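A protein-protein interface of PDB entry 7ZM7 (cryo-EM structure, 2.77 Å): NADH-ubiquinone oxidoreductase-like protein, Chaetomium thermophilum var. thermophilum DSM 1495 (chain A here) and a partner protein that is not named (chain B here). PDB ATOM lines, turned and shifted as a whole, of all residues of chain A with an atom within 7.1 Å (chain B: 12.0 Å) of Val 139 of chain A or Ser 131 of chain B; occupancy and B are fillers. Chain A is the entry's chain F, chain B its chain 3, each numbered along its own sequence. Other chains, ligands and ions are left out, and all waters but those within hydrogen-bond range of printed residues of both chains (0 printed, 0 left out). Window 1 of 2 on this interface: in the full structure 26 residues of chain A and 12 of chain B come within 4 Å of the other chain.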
ATOM      1  N   SER A  44       1.423 -21.818  11.836  1.00  0.00           N
ATOM      2  CA  SER A  44       2.297 -22.680  12.675  1.00  0.00           C
ATOM      3  C   SER A  44       1.504 -23.081  13.922  1.00  0.00           C
ATOM      4  O   SER A  44       1.675 -22.396  14.941  1.00  0.00           O
ATOM      5  CB  SER A  44       3.552 -21.939  13.056  1.00  0.00           C
ATOM      6  OG  SER A  44       3.247 -20.664  13.601  1.00  0.00           O
ATOM      7  N   SER A  47       3.791 -24.364  17.451  1.00  0.00           N
ATOM      8  CA  SER A  47       4.583 -23.386  18.164  1.00  0.00           C
ATOM      9  C   SER A  47       3.710 -22.301  18.762  1.00  0.00           C
ATOM     10  O   SER A  47       4.064 -21.734  19.797  1.00  0.00           O
ATOM     11  CB  SER A  47       5.631 -22.788  17.236  1.00  0.00           C
ATOM     12  OG  SER A  47       6.753 -23.637  17.134  1.00  0.00           O
ATOM     13  N   ALA A  48       2.587 -21.979  18.124  1.00  0.00           N
ATOM     14  CA  ALA A  48       1.679 -21.003  18.708  1.00  0.00           C
ATOM     15  C   ALA A  48       1.153 -21.508  20.033  1.00  0.00           C
ATOM     16  O   ALA A  48       1.140 -20.789  21.038  1.00  0.00           O
ATOM     17  CB  ALA A  48       0.525 -20.712  17.756  1.00  0.00           C
ATOM     18  N   TYR A  51       3.867 -21.393  22.631  1.00  0.00           N
ATOM     19  CA  TYR A  51       4.090 -20.023  23.068  1.00  0.00           C
ATOM     20  C   TYR A  51       3.026 -19.575  24.053  1.00  0.00           C
ATOM     21  O   TYR A  51       3.331 -18.906  25.043  1.00  0.00           O
ATOM     22  CB  TYR A  51       4.113 -19.107  21.852  1.00  0.00           C
ATOM     23  CG  TYR A  51       4.261 -17.649  22.177  1.00  0.00           C
ATOM     24  CD1 TYR A  51       5.519 -17.084  22.359  1.00  0.00           C
ATOM     25  CD2 TYR A  51       3.155 -16.832  22.298  1.00  0.00           C
ATOM     26  CE1 TYR A  51       5.666 -15.762  22.655  1.00  0.00           C
ATOM     27  CE2 TYR A  51       3.298 -15.513  22.592  1.00  0.00           C
ATOM     28  CZ  TYR A  51       4.557 -14.979  22.770  1.00  0.00           C
ATOM     29  OH  TYR A  51       4.692 -13.646  23.058  1.00  0.00           O
ATOM     30  N   TYR A  92      13.008 -31.519  12.958  1.00  0.00           N
ATOM     31  CA  TYR A  92      13.029 -30.464  13.960  1.00  0.00           C
ATOM     32  C   TYR A  92      14.400 -30.329  14.600  1.00  0.00           C
ATOM     33  O   TYR A  92      14.899 -29.214  14.771  1.00  0.00           O
ATOM     34  CB  TYR A  92      11.972 -30.725  15.028  1.00  0.00           C
ATOM     35  CG  TYR A  92      12.121 -29.832  16.235  1.00  0.00           C
ATOM     36  CD1 TYR A  92      11.893 -28.471  16.139  1.00  0.00           C
ATOM     37  CD2 TYR A  92      12.491 -30.346  17.462  1.00  0.00           C
ATOM     38  CE1 TYR A  92      12.027 -27.648  17.225  1.00  0.00           C
ATOM     39  CE2 TYR A  92      12.624 -29.528  18.558  1.00  0.00           C
ATOM     40  CZ  TYR A  92      12.391 -28.176  18.431  1.00  0.00           C
ATOM     41  OH  TYR A  92      12.524 -27.343  19.520  1.00  0.00           O
ATOM     42  N   TRP A  95      16.695 -28.628  12.180  1.00  0.00           N
ATOM     43  CA  TRP A  95      16.400 -27.218  11.989  1.00  0.00           C
ATOM     44  C   TRP A  95      16.798 -26.403  13.208  1.00  0.00           C
ATOM     45  O   TRP A  95      17.344 -25.304  13.071  1.00  0.00           O
ATOM     46  CB  TRP A  95      14.920 -27.012  11.658  1.00  0.00           C
ATOM     47  CG  TRP A  95      14.523 -25.596  11.829  1.00  0.00           C
ATOM     48  CD1 TRP A  95      14.636 -24.607  10.919  1.00  0.00           C
ATOM     49  CD2 TRP A  95      13.981 -24.995  13.005  1.00  0.00           C
ATOM     50  NE1 TRP A  95      14.198 -23.425  11.444  1.00  0.00           N
ATOM     51  CE2 TRP A  95      13.788 -23.642  12.728  1.00  0.00           C
ATOM     52  CE3 TRP A  95      13.645 -25.475  14.270  1.00  0.00           C
ATOM     53  CZ2 TRP A  95      13.273 -22.762  13.664  1.00  0.00           C
ATOM     54  CZ3 TRP A  95      13.142 -24.598  15.193  1.00  0.00           C
ATOM     55  CH2 TRP A  95      12.956 -23.259  14.888  1.00  0.00           C
ATOM     56  N   ALA A  99      19.081 -22.917  13.606  1.00  0.00           N
ATOM     57  CA  ALA A  99      18.408 -21.729  14.103  1.00  0.00           C
ATOM     58  C   ALA A  99      19.052 -21.214  15.378  1.00  0.00           C
ATOM     59  O   ALA A  99      19.075 -20.004  15.608  1.00  0.00           O
ATOM     60  CB  ALA A  99      16.933 -22.040  14.316  1.00  0.00           C
ATOM     61  N   LEU A 103      20.610 -17.409  15.311  1.00  0.00           N
ATOM     62  CA  LEU A 103      20.355 -16.404  16.340  1.00  0.00           C
ATOM     63  C   LEU A 103      21.635 -15.919  16.987  1.00  0.00           C
ATOM     64  O   LEU A 103      21.794 -14.720  17.231  1.00  0.00           O
ATOM     65  CB  LEU A 103      19.446 -16.969  17.425  1.00  0.00           C
ATOM     66  CG  LEU A 103      17.931 -16.880  17.366  1.00  0.00           C
ATOM     67  CD1 LEU A 103      17.428 -17.858  18.336  1.00  0.00           C
ATOM     68  CD2 LEU A 103      17.532 -15.504  17.813  1.00  0.00           C
ATOM     69  N   PHE A 110      17.490  -9.693  15.569  1.00  0.00           N
ATOM     70  CA  PHE A 110      16.203 -10.122  16.095  1.00  0.00           C
ATOM     71  C   PHE A 110      15.954  -9.648  17.524  1.00  0.00           C
ATOM     72  O   PHE A 110      15.389 -10.393  18.325  1.00  0.00           O
ATOM     73  CB  PHE A 110      16.083 -11.647  16.051  1.00  0.00           C
ATOM     74  CG  PHE A 110      16.658 -12.283  14.832  1.00  0.00           C
ATOM     75  CD1 PHE A 110      15.908 -12.404  13.683  1.00  0.00           C
ATOM     76  CD2 PHE A 110      17.932 -12.808  14.852  1.00  0.00           C
ATOM     77  CE1 PHE A 110      16.432 -13.019  12.549  1.00  0.00           C
ATOM     78  CE2 PHE A 110      18.457 -13.417  13.741  1.00  0.00           C
ATOM     79  CZ  PHE A 110      17.704 -13.523  12.584  1.00  0.00           C
ATOM     80  N   ARG A 127      10.429  -9.833   8.792  1.00  0.00           N
ATOM     81  CA  ARG A 127      10.601  -9.261  10.128  1.00  0.00           C
ATOM     82  C   ARG A 127      10.520 -10.395  11.145  1.00  0.00           C
ATOM     83  O   ARG A 127       9.537 -11.132  11.161  1.00  0.00           O
ATOM     84  CB  ARG A 127       9.542  -8.207  10.397  1.00  0.00           C
ATOM     85  CG  ARG A 127       9.728  -6.926   9.621  1.00  0.00           C
ATOM     86  CD  ARG A 127       8.506  -6.034   9.704  1.00  0.00           C
ATOM     87  NE  ARG A 127       7.273  -6.792   9.530  1.00  0.00           N
ATOM     88  CZ  ARG A 127       6.064  -6.329   9.830  1.00  0.00           C
ATOM     89  NH1 ARG A 127       5.924  -5.105  10.315  1.00  0.00           N
ATOM     90  NH2 ARG A 127       4.991  -7.086   9.644  1.00  0.00           N
ATOM     91  N   ALA A 128      11.548 -10.540  11.976  1.00  0.00           N
ATOM     92  CA  ALA A 128      11.572 -11.517  13.055  1.00  0.00           C
ATOM     93  C   ALA A 128      12.011 -10.846  14.347  1.00  0.00           C
ATOM     94  O   ALA A 128      12.575  -9.751  14.329  1.00  0.00           O
ATOM     95  CB  ALA A 128      12.506 -12.685  12.750  1.00  0.00           C
ATOM     96  N   VAL A 129      11.727 -11.491  15.473  1.00  0.00           N
ATOM     97  CA  VAL A 129      12.199 -10.999  16.761  1.00  0.00           C
ATOM     98  C   VAL A 129      12.274 -12.171  17.724  1.00  0.00           C
ATOM     99  O   VAL A 129      11.396 -13.034  17.734  1.00  0.00           O
ATOM    100  CB  VAL A 129      11.312  -9.854  17.309  1.00  0.00           C
ATOM    101  CG1 VAL A 129       9.868 -10.272  17.470  1.00  0.00           C
ATOM    102  CG2 VAL A 129      11.844  -9.370  18.630  1.00  0.00           C
ATOM    103  N   LYS A 130      13.336 -12.201  18.528  1.00  0.00           N
ATOM    104  CA  LYS A 130      13.512 -13.220  19.549  1.00  0.00           C
ATOM    105  C   LYS A 130      12.762 -12.806  20.802  1.00  0.00           C
ATOM    106  O   LYS A 130      12.940 -11.693  21.297  1.00  0.00           O
ATOM    107  CB  LYS A 130      14.984 -13.446  19.888  1.00  0.00           C
ATOM    108  CG  LYS A 130      15.160 -14.564  20.883  1.00  0.00           C
ATOM    109  CD  LYS A 130      16.591 -14.888  21.214  1.00  0.00           C
ATOM    110  CE  LYS A 130      17.182 -13.846  22.135  1.00  0.00           C
ATOM    111  NZ  LYS A 130      18.549 -14.222  22.567  1.00  0.00           N
ATOM    112  N   VAL A 131      11.921 -13.697  21.302  1.00  0.00           N
ATOM    113  CA  VAL A 131      11.085 -13.440  22.465  1.00  0.00           C
ATOM    114  C   VAL A 131      11.295 -14.575  23.450  1.00  0.00           C
ATOM    115  O   VAL A 131      11.387 -15.741  23.056  1.00  0.00           O
ATOM    116  CB  VAL A 131       9.598 -13.301  22.077  1.00  0.00           C
ATOM    117  CG1 VAL A 131       8.738 -13.039  23.281  1.00  0.00           C
ATOM    118  CG2 VAL A 131       9.435 -12.177  21.102  1.00  0.00           C
ATOM    119  N   VAL A 137      12.677 -20.089  24.242  1.00  0.00           N
ATOM    120  CA  VAL A 137      13.012 -19.110  23.219  1.00  0.00           C
ATOM    121  C   VAL A 137      12.079 -19.293  22.033  1.00  0.00           C
ATOM    122  O   VAL A 137      11.872 -20.415  21.564  1.00  0.00           O
ATOM    123  CB  VAL A 137      14.486 -19.224  22.802  1.00  0.00           C
ATOM    124  CG1 VAL A 137      14.810 -18.212  21.729  1.00  0.00           C
ATOM    125  CG2 VAL A 137      15.360 -19.006  24.001  1.00  0.00           C
ATOM    126  N   PHE A 138      11.509 -18.194  21.559  1.00  0.00           N
ATOM    127  CA  PHE A 138      10.669 -18.196  20.375  1.00  0.00           C
ATOM    128  C   PHE A 138      11.124 -17.091  19.441  1.00  0.00           C
ATOM    129  O   PHE A 138      11.671 -16.077  19.874  1.00  0.00           O
ATOM    130  CB  PHE A 138       9.182 -17.992  20.717  1.00  0.00           C
ATOM    131  CG  PHE A 138       8.673 -18.898  21.802  1.00  0.00           C
ATOM    132  CD1 PHE A 138       8.149 -20.135  21.502  1.00  0.00           C
ATOM    133  CD2 PHE A 138       8.722 -18.509  23.125  1.00  0.00           C
ATOM    134  CE1 PHE A 138       7.694 -20.954  22.480  1.00  0.00           C
ATOM    135  CE2 PHE A 138       8.255 -19.339  24.110  1.00  0.00           C
ATOM    136  CZ  PHE A 138       7.745 -20.563  23.783  1.00  0.00           C
ATOM    137  N   VAL A 139      10.905 -17.297  18.152  1.00  0.00           N
ATOM    138  CA  VAL A 139      11.062 -16.248  17.157  1.00  0.00           C
ATOM    139  C   VAL A 139       9.680 -15.962  16.605  1.00  0.00           C
ATOM    140  O   VAL A 139       8.944 -16.887  16.254  1.00  0.00           O
ATOM    141  CB  VAL A 139      12.040 -16.637  16.037  1.00  0.00           C
ATOM    142  CG1 VAL A 139      12.131 -15.520  15.024  1.00  0.00           C
ATOM    143  CG2 VAL A 139      13.394 -16.915  16.601  1.00  0.00           C
ATOM    144  N   VAL A 140       9.308 -14.694  16.576  1.00  0.00           N
ATOM    145  CA  VAL A 140       8.038 -14.268  16.015  1.00  0.00           C
ATOM    146  C   VAL A 140       8.359 -13.583  14.695  1.00  0.00           C
ATOM    147  O   VAL A 140       8.776 -12.426  14.658  1.00  0.00           O
ATOM    148  CB  VAL A 140       7.266 -13.358  16.974  1.00  0.00           C
ATOM    149  CG1 VAL A 140       5.844 -13.219  16.518  1.00  0.00           C
ATOM    150  CG2 VAL A 140       7.300 -13.926  18.381  1.00  0.00           C
ATOM    151  N   SER A 141       8.178 -14.306  13.608  1.00  0.00           N
ATOM    152  CA  SER A 141       8.454 -13.796  12.279  1.00  0.00           C
ATOM    153  C   SER A 141       7.142 -13.381  11.622  1.00  0.00           C
ATOM    154  O   SER A 141       6.209 -14.181  11.528  1.00  0.00           O
ATOM    155  CB  SER A 141       9.178 -14.849  11.445  1.00  0.00           C
ATOM    156  OG  SER A 141       9.755 -14.285  10.288  1.00  0.00           O
ATOM    157  N   TRP A 196      15.999 -15.374   8.287  1.00  0.00           N
ATOM    158  CA  TRP A 196      15.501 -16.337   9.248  1.00  0.00           C
ATOM    159  C   TRP A 196      14.693 -17.413   8.535  1.00  0.00           C
ATOM    160  O   TRP A 196      13.746 -17.110   7.806  1.00  0.00           O
ATOM    161  CB  TRP A 196      14.645 -15.635  10.295  1.00  0.00           C
ATOM    162  CG  TRP A 196      13.868 -16.567  11.138  1.00  0.00           C
ATOM    163  CD1 TRP A 196      12.542 -16.795  11.079  1.00  0.00           C
ATOM    164  CD2 TRP A 196      14.376 -17.409  12.173  1.00  0.00           C
ATOM    165  NE1 TRP A 196      12.175 -17.724  12.012  1.00  0.00           N
ATOM    166  CE2 TRP A 196      13.288 -18.121  12.699  1.00  0.00           C
ATOM    167  CE3 TRP A 196      15.644 -17.631  12.701  1.00  0.00           C
ATOM    168  CZ2 TRP A 196      13.425 -19.039  13.737  1.00  0.00           C
ATOM    169  CZ3 TRP A 196      15.783 -18.537  13.722  1.00  0.00           C
ATOM    170  CH2 TRP A 196      14.679 -19.236  14.233  1.00  0.00           C
ATOM    171  N   GLU A 197      15.067 -18.674   8.748  1.00  0.00           N
ATOM    172  CA  GLU A 197      14.374 -19.795   8.133  1.00  0.00           C
ATOM    173  C   GLU A 197      13.318 -20.324   9.078  1.00  0.00           C
ATOM    174  O   GLU A 197      13.602 -20.499  10.270  1.00  0.00           O
ATOM    175  CB  GLU A 197      15.351 -20.906   7.783  1.00  0.00           C
ATOM    176  CG  GLU A 197      14.726 -22.090   7.094  1.00  0.00           C
ATOM    177  CD  GLU A 197      15.526 -23.355   7.295  1.00  0.00           C
ATOM    178  OE1 GLU A 197      16.706 -23.253   7.688  1.00  0.00           O
ATOM    179  OE2 GLU A 197      14.974 -24.449   7.072  1.00  0.00           O
ATOM    180  N   PRO A 198      12.107 -20.588   8.598  1.00  0.00           N
ATOM    181  CA  PRO A 198      11.026 -20.979   9.501  1.00  0.00           C
ATOM    182  C   PRO A 198      11.203 -22.389  10.042  1.00  0.00           C
ATOM    183  O   PRO A 198      11.953 -23.207   9.511  1.00  0.00           O
ATOM    184  CB  PRO A 198       9.785 -20.886   8.612  1.00  0.00           C
ATOM    185  CG  PRO A 198      10.309 -21.153   7.249  1.00  0.00           C
ATOM    186  CD  PRO A 198      11.654 -20.524   7.200  1.00  0.00           C
ATOM    187  N   GLU A 199      10.490 -22.654  11.128  1.00  0.00           N
ATOM    188  CA  GLU A 199      10.466 -23.976  11.732  1.00  0.00           C
ATOM    189  C   GLU A 199       9.719 -24.956  10.826  1.00  0.00           C
ATOM    190  O   GLU A 199       8.787 -24.563  10.124  1.00  0.00           O
ATOM    191  CB  GLU A 199       9.787 -23.900  13.103  1.00  0.00           C
ATOM    192  CG  GLU A 199       9.994 -25.103  13.980  1.00  0.00           C
ATOM    193  CD  GLU A 199       9.661 -24.845  15.425  1.00  0.00           C
ATOM    194  OE1 GLU A 199      10.025 -25.670  16.280  1.00  0.00           O
ATOM    195  OE2 GLU A 199       9.013 -23.830  15.717  1.00  0.00           O
ATOM    196  N   SER B 126      -2.818 -15.650   8.542  1.00  0.00           N
ATOM    197  CA  SER B 126      -2.196 -14.710   9.463  1.00  0.00           C
ATOM    198  C   SER B 126      -0.705 -14.614   9.179  1.00  0.00           C
ATOM    199  O   SER B 126      -0.047 -15.630   8.946  1.00  0.00           O
ATOM    200  CB  SER B 126      -2.430 -15.133  10.914  1.00  0.00           C
ATOM    201  OG  SER B 126      -1.684 -14.324  11.808  1.00  0.00           O
ATOM    202  N   SER B 127      -0.177 -13.389   9.214  1.00  0.00           N
ATOM    203  CA  SER B 127       1.242 -13.184   8.950  1.00  0.00           C
ATOM    204  C   SER B 127       2.098 -13.575  10.145  1.00  0.00           C
ATOM    205  O   SER B 127       3.303 -13.793  10.006  1.00  0.00           O
ATOM    206  CB  SER B 127       1.495 -11.730   8.573  1.00  0.00           C
ATOM    207  OG  SER B 127       0.533 -11.277   7.639  1.00  0.00           O
ATOM    208  N   VAL B 128       1.500 -13.667  11.329  1.00  0.00           N
ATOM    209  CA  VAL B 128       2.258 -13.916  12.551  1.00  0.00           C
ATOM    210  C   VAL B 128       2.567 -15.408  12.633  1.00  0.00           C
ATOM    211  O   VAL B 128       1.655 -16.227  12.767  1.00  0.00           O
ATOM    212  CB  VAL B 128       1.492 -13.438  13.788  1.00  0.00           C
ATOM    213  CG1 VAL B 128       2.281 -13.731  15.048  1.00  0.00           C
ATOM    214  CG2 VAL B 128       1.179 -11.969  13.676  1.00  0.00           C
ATOM    215  N   VAL B 129       3.844 -15.765  12.553  1.00  0.00           N
ATOM    216  CA  VAL B 129       4.287 -17.153  12.549  1.00  0.00           C
ATOM    217  C   VAL B 129       5.299 -17.336  13.667  1.00  0.00           C
ATOM    218  O   VAL B 129       6.317 -16.639  13.705  1.00  0.00           O
ATOM    219  CB  VAL B 129       4.900 -17.551  11.204  1.00  0.00           C
ATOM    220  CG1 VAL B 129       5.432 -18.963  11.275  1.00  0.00           C
ATOM    221  CG2 VAL B 129       3.891 -17.415  10.115  1.00  0.00           C
ATOM    222  N   ILE B 130       5.032 -18.273  14.564  1.00  0.00           N
ATOM    223  CA  ILE B 130       5.880 -18.481  15.728  1.00  0.00           C
ATOM    224  C   ILE B 130       6.712 -19.732  15.535  1.00  0.00           C
ATOM    225  O   ILE B 130       6.285 -20.715  14.927  1.00  0.00           O
ATOM    226  CB  ILE B 130       5.077 -18.556  17.039  1.00  0.00           C
ATOM    227  CG1 ILE B 130       3.992 -17.497  17.061  1.00  0.00           C
ATOM    228  CG2 ILE B 130       5.982 -18.323  18.223  1.00  0.00           C
ATOM    229  CD1 ILE B 130       2.961 -17.748  18.112  1.00  0.00           C
ATOM    230  N   SER B 131       7.929 -19.678  16.061  1.00  0.00           N
ATOM    231  CA  SER B 131       8.881 -20.767  15.991  1.00  0.00           C
ATOM    232  C   SER B 131       9.311 -21.119  17.397  1.00  0.00           C
ATOM    233  O   SER B 131       9.505 -20.233  18.227  1.00  0.00           O
ATOM    234  CB  SER B 131      10.096 -20.381  15.157  1.00  0.00           C
ATOM    235  OG  SER B 131       9.707 -19.733  13.966  1.00  0.00           O
ATOM    236  N   TYR B 132       9.455 -22.405  17.673  1.00  0.00           N
ATOM    237  CA  TYR B 132       9.888 -22.855  18.986  1.00  0.00           C
ATOM    238  C   TYR B 132      11.345 -23.273  18.916  1.00  0.00           C
ATOM    239  O   TYR B 132      11.728 -24.065  18.054  1.00  0.00           O
ATOM    240  CB  TYR B 132       9.031 -24.006  19.499  1.00  0.00           C
ATOM    241  CG  TYR B 132       9.467 -24.516  20.841  1.00  0.00           C
ATOM    242  CD1 TYR B 132       9.536 -23.658  21.934  1.00  0.00           C
ATOM    243  CD2 TYR B 132       9.803 -25.839  21.030  1.00  0.00           C
ATOM    244  CE1 TYR B 132       9.924 -24.091  23.159  1.00  0.00           C
ATOM    245  CE2 TYR B 132      10.200 -26.287  22.274  1.00  0.00           C
ATOM    246  CZ  TYR B 132      10.253 -25.398  23.332  1.00  0.00           C
ATOM    247  OH  TYR B 132      10.642 -25.820  24.572  1.00  0.00           O
ATOM    248  N   LEU B 133      12.144 -22.748  19.837  1.00  0.00           N
ATOM    249  CA  LEU B 133      13.571 -23.006  19.880  1.00  0.00           C
ATOM    250  C   LEU B 133      14.003 -23.851  21.060  1.00  0.00           C
ATOM    251  O   LEU B 133      15.058 -24.482  20.987  1.00  0.00           O
ATOM    252  CB  LEU B 133      14.328 -21.674  19.889  1.00  0.00           C
ATOM    253  CG  LEU B 133      14.096 -21.011  18.538  1.00  0.00           C
ATOM    254  CD1 LEU B 133      14.499 -19.594  18.553  1.00  0.00           C
ATOM    255  CD2 LEU B 133      14.955 -21.727  17.532  1.00  0.00           C
ATOM    256  N   GLY B 134      13.222 -23.900  22.120  1.00  0.00           N
ATOM    257  CA  GLY B 134      13.555 -24.692  23.271  1.00  0.00           C
ATOM    258  C   GLY B 134      14.037 -23.866  24.442  1.00  0.00           C
ATOM    259  O   GLY B 134      13.876 -22.650  24.512  1.00  0.00           O
ATOM    260  N   ASN B 135      14.652 -24.570  25.383  1.00  0.00           N
ATOM    261  CA  ASN B 135      15.176 -23.958  26.588  1.00  0.00           C
ATOM    262  C   ASN B 135      16.385 -23.088  26.265  1.00  0.00           C
ATOM    263  O   ASN B 135      16.974 -23.171  25.186  1.00  0.00           O
ATOM    264  CB  ASN B 135      15.560 -25.038  27.599  1.00  0.00           C
ATOM    265  CG  ASN B 135      15.289 -24.625  29.026  1.00  0.00           C
ATOM    266  OD1 ASN B 135      15.490 -23.470  29.400  1.00  0.00           O
ATOM    267  ND2 ASN B 135      14.847 -25.573  29.842  1.00  0.00           N
ATOM    268  N   ILE B 136      16.754 -22.248  27.222  1.00  0.00           N
ATOM    269  CA  ILE B 136      17.930 -21.401  27.077  1.00  0.00           C
ATOM    270  C   ILE B 136      19.196 -22.199  27.351  1.00  0.00           C
ATOM    271  O   ILE B 136      20.176 -22.101  26.612  1.00  0.00           O
ATOM    272  CB  ILE B 136      17.845 -20.186  27.999  1.00  0.00           C
ATOM    273  CG1 ILE B 136      16.612 -19.355  27.657  1.00  0.00           C
ATOM    274  CG2 ILE B 136      19.095 -19.343  27.873  1.00  0.00           C
ATOM    275  CD1 ILE B 136      16.282 -18.317  28.696  1.00  0.00           C
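The side-chain carboxylate of Glu 199 of chain A sits at hydrogen-bond distance from the side-chain hydroxyl of Ser 47 of chain A. The backbone carbonyl oxygen (O) of Glu 197 of chain A lies within hydrogen-bond range of the indole nitrogen (NE1) of Trp 95 of chain A (3.2 Å). The backbone carbonyl oxygen of Pro 198 of chain A lies within hydrogen-bond range of the indole nitrogen of Trp 95 of chain A, at 3.0 Å. The backbone NH (N) of Val 140 of chain A is in hydrogen-bond range of the backbone carbonyl oxygen (O) of Val 129 of chain A (2.9 Å). The backbone carbonyl oxygen (O) of Phe 138 of chain A sits at hydrogen-bond distance from the backbone NH (N) of Val 131 of chain A (2.8 Å). OG of Ser 126 of chain B sits close to N of Val 128 of chain B, at 3.3 Å.
Among the printed residues, merely in contact across the chains: Glu 199 of chain A with Ser 131 of chain B (3.1 Å), Ser 47 of chain A with Ile 130 of chain B (3.2 Å), Phe 138 of chain A with Ser 131 of chain B (3.2 Å), Trp 95 of chain A with Tyr 132 of chain B (3.2 Å), Phe 138 of chain A with Tyr 132 of chain B (3.3 Å), Leu 103 of chain A with Leu 133 of chain B (3.4 Å), Tyr 92 of chain A with Tyr 132 of chain B (3.5 Å), Val 139 of chain A with Ile 130 of chain B (3.5 Å), Val 139 of chain A with Leu 133 of chain B (3.5 Å), Ala 48 of chain A with Ile 130 of chain B (3.5 Å), Ser 47 of chain A with Ser 131 of chain B (3.6 Å), Ser 44 of chain A with Val 129 of chain B (3.6 Å), Trp 95 of chain A with Leu 133 of chain B (3.7 Å), Val 139 of chain A with Val 129 of chain B (3.7 Å), Val 140 of chain A with Val 129 of chain B (3.7 Å), Trp 196 of chain A with Ser 131 of chain B (3.7 Å), Ala 99 of chain A with Leu 133 of chain B (3.8 Å), Val 137 of chain A with Ile 136 of chain B (3.9 Å), Val 140 of chain A with Val 128 of chain B (3.9 Å), Val 137 of chain A with Tyr 132 of chain B (3.9 Å) and Ser 141 of chain A with Val 128 of chain B (3.999 Å).
Of the 11 printed residues of chain B, 9 touch a printed residue of chain A. Hydrophobic or aromatic side chains of chain B that line the printed part of chain A: Val 128, Val 129, Ile 130, Tyr 132, Leu 133 and Ile 136. Printed residues of chain A that touch a printed residue of chain B: Ser 44, Ser 47, Ala 48, Tyr 92, Trp 95, Ala 99, Leu 103, Val 137, Phe 138, Val 139, Val 140, Ser 141, Trp 196 and Glu 199. Hydrophobic or aromatic side chains of chain A that line the printed part of chain B: Ala 48, Tyr 92, Trp 95, Ala 99, Leu 103, Val 137, Phe 138, Val 139, Val 140 and Trp 196. Among the printed residues, 29 pairs touch across the chains.
Of chain B, only Val 129 (3.7 Å), Ile 130 (3.5 Å), Ser 131 (3.0 Å) and Leu 133 (3.5 Å) come within 4 Å of Val 139 of chain A. Of the printed residues of chain A, Ser 131 of chain B touches Ser 47 (3.6 Å), Phe 138 (3.2 Å), Val 139 (3.0 Å), Trp 196 (3.7 Å) and Glu 199 (3.1 Å). No residue of chain B comes within 4 Å of Val 129 of chain A. No residue of chain B comes within 4 Å of Val 131 of chain A. Val 140 of chain A touches two residues of chain B. Printed residues of chain B within 4 Å of Trp 196 of chain A: Ser 131 (3.7 Å). Glu 199 of chain A touches just these residues of chain B: Ser 131 and Tyr 132. Of the printed residues of chain B, Ala 99 of chain A touches Leu 133 (3.8 Å). Printed residues of chain B within 4 Å of Ser 141 of chain A: Ser 127, Val 128 and Val 129. The nearest residue of chain B that does not touch Val 139 of chain A is Tyr 132 of chain B (5.3 Å). The nearest printed residue of chain A that does not touch Ser 131 of chain B is Trp 95 of chain A (4.1 Å).
OG of Ser 44 of chain A lies within hydrogen-bond range of N of Ile 130 of chain B (3.1 Å). The side-chain hydroxyl (OG) of Ser 47 of chain A sits at hydrogen-bond distance from the backbone NH (N) of Tyr 132 of chain B. The backbone NH (N) of Leu 133 of chain B is in hydrogen-bond range of the backbone carbonyl oxygen (O) of Val 137 of chain A (2.9 Å). The backbone NH (N) of Val 137 of chain A lies within hydrogen-bond range of the backbone carbonyl oxygen (O) of Gly 134 of chain B (2.8 Å). O of Val 139 of chain A is in hydrogen-bond range of N of Ser 131 of chain B. The backbone carbonyl oxygen (O) of Val 129 of chain B is in hydrogen-bond range of the backbone NH (N) of Ser 141 of chain A, at 3.0 Å. The side-chain carboxylate (OE2) of Glu 199 of chain A is in hydrogen-bond range of the backbone NH (N) of Tyr 132 of chain B (2.5 Å). O of Ser 127 of chain B lies close to O of Ser 141 of chain A (3.3 Å).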
